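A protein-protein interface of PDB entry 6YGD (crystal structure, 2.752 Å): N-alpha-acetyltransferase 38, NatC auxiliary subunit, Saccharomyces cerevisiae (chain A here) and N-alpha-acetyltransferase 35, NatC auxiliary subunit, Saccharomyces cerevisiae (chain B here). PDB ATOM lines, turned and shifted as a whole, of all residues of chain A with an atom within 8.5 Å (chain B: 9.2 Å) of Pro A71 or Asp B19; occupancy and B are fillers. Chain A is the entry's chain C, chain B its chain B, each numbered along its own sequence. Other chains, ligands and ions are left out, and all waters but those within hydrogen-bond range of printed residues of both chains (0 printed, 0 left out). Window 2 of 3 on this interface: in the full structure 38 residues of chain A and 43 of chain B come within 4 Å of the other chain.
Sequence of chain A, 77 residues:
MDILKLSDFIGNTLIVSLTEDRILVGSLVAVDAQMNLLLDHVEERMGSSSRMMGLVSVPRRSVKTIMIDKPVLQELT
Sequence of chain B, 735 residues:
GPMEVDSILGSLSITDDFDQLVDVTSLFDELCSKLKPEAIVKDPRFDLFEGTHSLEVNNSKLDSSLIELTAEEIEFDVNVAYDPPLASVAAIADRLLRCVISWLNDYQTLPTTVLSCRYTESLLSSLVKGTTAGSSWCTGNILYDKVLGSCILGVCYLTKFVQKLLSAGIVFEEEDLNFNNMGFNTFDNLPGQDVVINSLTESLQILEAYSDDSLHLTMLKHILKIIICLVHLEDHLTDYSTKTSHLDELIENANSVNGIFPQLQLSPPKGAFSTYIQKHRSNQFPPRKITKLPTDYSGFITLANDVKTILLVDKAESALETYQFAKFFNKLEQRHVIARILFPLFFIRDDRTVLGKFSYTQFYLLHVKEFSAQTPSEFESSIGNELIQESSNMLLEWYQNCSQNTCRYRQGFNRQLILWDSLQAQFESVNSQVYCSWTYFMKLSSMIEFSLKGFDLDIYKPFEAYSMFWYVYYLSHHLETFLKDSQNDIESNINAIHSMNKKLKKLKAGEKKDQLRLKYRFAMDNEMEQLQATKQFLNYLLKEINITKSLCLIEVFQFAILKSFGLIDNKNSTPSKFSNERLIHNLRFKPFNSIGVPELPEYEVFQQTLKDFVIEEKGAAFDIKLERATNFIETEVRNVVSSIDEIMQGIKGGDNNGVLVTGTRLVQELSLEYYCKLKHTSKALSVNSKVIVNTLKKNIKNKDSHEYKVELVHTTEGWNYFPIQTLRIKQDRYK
Pro A71 touches just one residue of chain B: Asp B19 (3.9 Å).
Thr B15 touches none of the printed residues of chain A.
Of the printed residues of chain A, Phe B18 touches Asp A69.
Of chain A, only Asp A69 (2.9 Å) and Pro A71 (3.9 Å) come within 4 Å of Asp B19.
Of the printed residues of chain A, Val B22 touches Ile A68 (2.9 Å) and Lys A70 (3.6 Å).
The nearest residue of chain A that does not touch Asp B19 is Lys A70 (5.6 Å).
O of Ile A68 touches O of Gln B20, 3.9 Å away.
CA of Leu B21 touches O of Ile A68 (3.4 Å).
CB of Phe B18 touches OD1 of Asp A69, 3.9 Å away.
N of Asp A69 touches CD2 of Leu B21 (3.7 Å).
Lys A70 touches Val B22 (CB to CG2, 3.6 Å).
CG of Pro A71 touches OD2 of Asp B19, 3.9 Å away.
N of Lys A70 is in hydrogen-bond range of O of Gln B20 (2.7 Å).
The backbone NH (N) of Val B22 is in hydrogen-bond range of the backbone carbonyl oxygen (O) of Ile A68, at 2.9 Å.
The side-chain carboxylate of Asp A69 lies close to the side-chain carboxylate of Asp B19.
OD1 of Asp A69 lies close to O of Gln B20, at 3.1 Å.
NZ of Lys A70 lies within hydrogen-bond range of OE1 of Gln A74, at 2.8 Å.
Printed residues of chain A that touch a printed residue of chain B: Ile A68, Asp A69, Lys A70 and Pro A71.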
ATOM      1  N   ILE A  68     -25.968  28.633  -7.101  1.00  0.00           N
ATOM      2  CA  ILE A  68     -27.291  28.073  -6.863  1.00  0.00           C
ATOM      3  C   ILE A  68     -27.162  27.005  -5.788  1.00  0.00           C
ATOM      4  O   ILE A  68     -26.125  26.343  -5.662  1.00  0.00           O
ATOM      5  CB  ILE A  68     -27.921  27.489  -8.152  1.00  0.00           C
ATOM      6  CG1 ILE A  68     -29.398  27.151  -7.933  1.00  0.00           C
ATOM      7  CG2 ILE A  68     -27.176  26.248  -8.601  1.00  0.00           C
ATOM      8  CD1 ILE A  68     -30.055  26.483  -9.120  1.00  0.00           C
ATOM      9  N   ASP A  69     -28.215  26.855  -4.990  1.00  0.00           N
ATOM     10  CA  ASP A  69     -28.251  25.793  -3.995  1.00  0.00           C
ATOM     11  C   ASP A  69     -28.233  24.441  -4.697  1.00  0.00           C
ATOM     12  O   ASP A  69     -29.071  24.176  -5.566  1.00  0.00           O
ATOM     13  CB  ASP A  69     -29.497  25.942  -3.121  1.00  0.00           C
ATOM     14  CG  ASP A  69     -29.500  24.993  -1.939  1.00  0.00           C
ATOM     15  OD1 ASP A  69     -28.517  24.993  -1.166  1.00  0.00           O
ATOM     16  OD2 ASP A  69     -30.493  24.255  -1.775  1.00  0.00           O
ATOM     17  N   LYS A  70     -27.265  23.596  -4.336  1.00  0.00           N
ATOM     18  CA  LYS A  70     -27.116  22.315  -5.022  1.00  0.00           C
ATOM     19  C   LYS A  70     -28.376  21.458  -4.976  1.00  0.00           C
ATOM     20  O   LYS A  70     -28.714  20.863  -6.015  1.00  0.00           O
ATOM     21  CB  LYS A  70     -25.914  21.546  -4.458  1.00  0.00           C
ATOM     22  CG  LYS A  70     -25.726  20.174  -5.095  1.00  0.00           C
ATOM     23  CD  LYS A  70     -24.334  19.616  -4.860  1.00  0.00           C
ATOM     24  CE  LYS A  70     -24.154  18.283  -5.567  1.00  0.00           C
ATOM     25  NZ  LYS A  70     -24.423  18.401  -7.026  1.00  0.00           N
ATOM     26  N   PRO A  71     -29.099  21.335  -3.854  1.00  0.00           N
ATOM     27  CA  PRO A  71     -30.393  20.634  -3.913  1.00  0.00           C
ATOM     28  C   PRO A  71     -31.341  21.205  -4.955  1.00  0.00           C
ATOM     29  O   PRO A  71     -31.842  20.459  -5.804  1.00  0.00           O
ATOM     30  CB  PRO A  71     -30.930  20.794  -2.484  1.00  0.00           C
ATOM     31  CG  PRO A  71     -29.710  20.871  -1.647  1.00  0.00           C
ATOM     32  CD  PRO A  71     -28.713  21.644  -2.464  1.00  0.00           C
ATOM     33  N   VAL A  72     -31.586  22.520  -4.923  1.00  0.00           N
ATOM     34  CA  VAL A  72     -32.473  23.149  -5.901  1.00  0.00           C
ATOM     35  C   VAL A  72     -31.943  22.957  -7.315  1.00  0.00           C
ATOM     36  O   VAL A  72     -32.723  22.817  -8.266  1.00  0.00           O
ATOM     37  CB  VAL A  72     -32.659  24.641  -5.562  1.00  0.00           C
ATOM     38  CG1 VAL A  72     -33.695  25.274  -6.480  1.00  0.00           C
ATOM     39  CG2 VAL A  72     -33.055  24.811  -4.103  1.00  0.00           C
ATOM     40  N   LEU A  73     -30.618  22.946  -7.479  1.00  0.00           N
ATOM     41  CA  LEU A  73     -30.030  22.670  -8.787  1.00  0.00           C
ATOM     42  C   LEU A  73     -30.410  21.276  -9.272  1.00  0.00           C
ATOM     43  O   LEU A  73     -30.829  21.096 -10.421  1.00  0.00           O
ATOM     44  CB  LEU A  73     -28.509  22.820  -8.716  1.00  0.00           C
ATOM     45  CG  LEU A  73     -27.721  22.554 -10.001  1.00  0.00           C
ATOM     46  CD1 LEU A  73     -28.053  23.599 -11.054  1.00  0.00           C
ATOM     47  CD2 LEU A  73     -26.225  22.520  -9.723  1.00  0.00           C
ATOM     48  N   GLN A  74     -30.274  20.274  -8.400  1.00  0.00           N
ATOM     49  CA  GLN A  74     -30.616  18.909  -8.785  1.00  0.00           C
ATOM     50  C   GLN A  74     -32.125  18.704  -8.850  1.00  0.00           C
ATOM     51  O   GLN A  74     -32.596  17.829  -9.586  1.00  0.00           O
ATOM     52  CB  GLN A  74     -29.987  17.912  -7.810  1.00  0.00           C
ATOM     53  CG  GLN A  74     -28.489  18.103  -7.582  1.00  0.00           C
ATOM     54  CD  GLN A  74     -27.649  17.745  -8.794  1.00  0.00           C
ATOM     55  OE1 GLN A  74     -26.520  18.216  -8.940  1.00  0.00           O
ATOM     56  NE2 GLN A  74     -28.190  16.901  -9.666  1.00  0.00           N
ATOM     57  N   GLU A  75     -32.892  19.485  -8.096  1.00  0.00           N
ATOM     58  CA  GLU A  75     -34.349  19.384  -8.111  1.00  0.00           C
ATOM     59  C   GLU A  75     -34.911  19.723  -9.488  1.00  0.00           C
ATOM     60  O   GLU A  75     -34.386  20.588 -10.188  1.00  0.00           O
ATOM     61  CB  GLU A  75     -34.964  20.305  -7.054  1.00  0.00           C
ATOM     62  CG  GLU A  75     -34.839  19.792  -5.626  1.00  0.00           C
ATOM     63  CD  GLU A  75     -34.961  20.899  -4.595  1.00  0.00           C
ATOM     64  OE1 GLU A  75     -35.505  21.973  -4.934  1.00  0.00           O
ATOM     65  OE2 GLU A  75     -34.503  20.700  -3.449  1.00  0.00           O
ATOM     66  N   THR B  15     -24.286  32.916   3.799  1.00  0.00           N
ATOM     67  CA  THR B  15     -24.987  31.842   3.106  1.00  0.00           C
ATOM     68  C   THR B  15     -25.130  30.597   3.977  1.00  0.00           C
ATOM     69  O   THR B  15     -25.086  29.474   3.471  1.00  0.00           O
ATOM     70  CB  THR B  15     -24.273  31.486   1.804  1.00  0.00           C
ATOM     71  OG1 THR B  15     -23.142  30.654   2.092  1.00  0.00           O
ATOM     72  CG2 THR B  15     -23.795  32.743   1.094  1.00  0.00           C
ATOM     73  N   ASP B  16     -25.299  30.778   5.290  1.00  0.00           N
ATOM     74  CA  ASP B  16     -25.431  29.622   6.172  1.00  0.00           C
ATOM     75  C   ASP B  16     -26.771  28.920   5.993  1.00  0.00           C
ATOM     76  O   ASP B  16     -26.870  27.712   6.238  1.00  0.00           O
ATOM     77  CB  ASP B  16     -25.239  30.038   7.631  1.00  0.00           C
ATOM     78  CG  ASP B  16     -23.781  30.017   8.058  1.00  0.00           C
ATOM     79  OD1 ASP B  16     -22.901  29.965   7.173  1.00  0.00           O
ATOM     80  OD2 ASP B  16     -23.517  30.045   9.280  1.00  0.00           O
ATOM     81  N   ASP B  17     -27.808  29.648   5.568  1.00  0.00           N
ATOM     82  CA  ASP B  17     -29.099  29.014   5.326  1.00  0.00           C
ATOM     83  C   ASP B  17     -29.079  28.116   4.096  1.00  0.00           C
ATOM     84  O   ASP B  17     -29.978  27.284   3.937  1.00  0.00           O
ATOM     85  CB  ASP B  17     -30.199  30.070   5.191  1.00  0.00           C
ATOM     86  CG  ASP B  17     -29.858  31.147   4.180  1.00  0.00           C
ATOM     87  OD1 ASP B  17     -28.706  31.627   4.181  1.00  0.00           O
ATOM     88  OD2 ASP B  17     -30.746  31.518   3.385  1.00  0.00           O
ATOM     89  N   PHE B  18     -28.080  28.262   3.229  1.00  0.00           N
ATOM     90  CA  PHE B  18     -27.895  27.383   2.083  1.00  0.00           C
ATOM     91  C   PHE B  18     -26.781  26.395   2.410  1.00  0.00           C
ATOM     92  O   PHE B  18     -25.637  26.799   2.642  1.00  0.00           O
ATOM     93  CB  PHE B  18     -27.557  28.180   0.825  1.00  0.00           C
ATOM     94  CG  PHE B  18     -28.511  29.303   0.545  1.00  0.00           C
ATOM     95  CD1 PHE B  18     -29.794  29.044   0.092  1.00  0.00           C
ATOM     96  CD2 PHE B  18     -28.121  30.619   0.729  1.00  0.00           C
ATOM     97  CE1 PHE B  18     -30.674  30.080  -0.168  1.00  0.00           C
ATOM     98  CE2 PHE B  18     -28.995  31.657   0.471  1.00  0.00           C
ATOM     99  CZ  PHE B  18     -30.274  31.387   0.022  1.00  0.00           C
ATOM    100  N   ASP B  19     -27.121  25.106   2.428  1.00  0.00           N
ATOM    101  CA  ASP B  19     -26.158  24.094   2.848  1.00  0.00           C
ATOM    102  C   ASP B  19     -25.017  23.957   1.845  1.00  0.00           C
ATOM    103  O   ASP B  19     -23.843  23.896   2.231  1.00  0.00           O
ATOM    104  CB  ASP B  19     -26.866  22.753   3.052  1.00  0.00           C
ATOM    105  CG  ASP B  19     -27.920  22.484   1.997  1.00  0.00           C
ATOM    106  OD1 ASP B  19     -28.182  23.385   1.173  1.00  0.00           O
ATOM    107  OD2 ASP B  19     -28.488  21.371   1.994  1.00  0.00           O
ATOM    108  N   GLN B  20     -25.337  23.911   0.553  1.00  0.00           N
ATOM    109  CA  GLN B  20     -24.334  23.666  -0.477  1.00  0.00           C
ATOM    110  C   GLN B  20     -24.631  24.543  -1.683  1.00  0.00           C
ATOM    111  O   GLN B  20     -25.708  24.438  -2.278  1.00  0.00           O
ATOM    112  CB  GLN B  20     -24.310  22.187  -0.874  1.00  0.00           C
ATOM    113  CG  GLN B  20     -23.076  21.767  -1.649  1.00  0.00           C
ATOM    114  CD  GLN B  20     -22.983  20.263  -1.823  1.00  0.00           C
ATOM    115  OE1 GLN B  20     -23.925  19.532  -1.514  1.00  0.00           O
ATOM    116  NE2 GLN B  20     -21.845  19.793  -2.319  1.00  0.00           N
ATOM    117  N   LEU B  21     -23.678  25.398  -2.041  1.00  0.00           N
ATOM    118  CA  LEU B  21     -23.803  26.300  -3.176  1.00  0.00           C
ATOM    119  C   LEU B  21     -22.815  25.900  -4.262  1.00  0.00           C
ATOM    120  O   LEU B  21     -21.668  25.548  -3.970  1.00  0.00           O
ATOM    121  CB  LEU B  21     -23.564  27.752  -2.752  1.00  0.00           C
ATOM    122  CG  LEU B  21     -24.607  28.345  -1.803  1.00  0.00           C
ATOM    123  CD1 LEU B  21     -24.257  29.778  -1.432  1.00  0.00           C
ATOM    124  CD2 LEU B  21     -25.987  28.277  -2.432  1.00  0.00           C
ATOM    125  N   VAL B  22     -23.262  25.954  -5.515  1.00  0.00           N
ATOM    126  CA  VAL B  22     -22.469  25.525  -6.660  1.00  0.00           C
ATOM    127  C   VAL B  22     -22.269  26.709  -7.596  1.00  0.00           C
ATOM    128  O   VAL B  22     -23.207  27.472  -7.852  1.00  0.00           O
ATOM    129  CB  VAL B  22     -23.138  24.346  -7.401  1.00  0.00           C
ATOM    130  CG1 VAL B  22     -22.252  23.851  -8.532  1.00  0.00           C
ATOM    131  CG2 VAL B  22     -23.442  23.219  -6.431  1.00  0.00           C
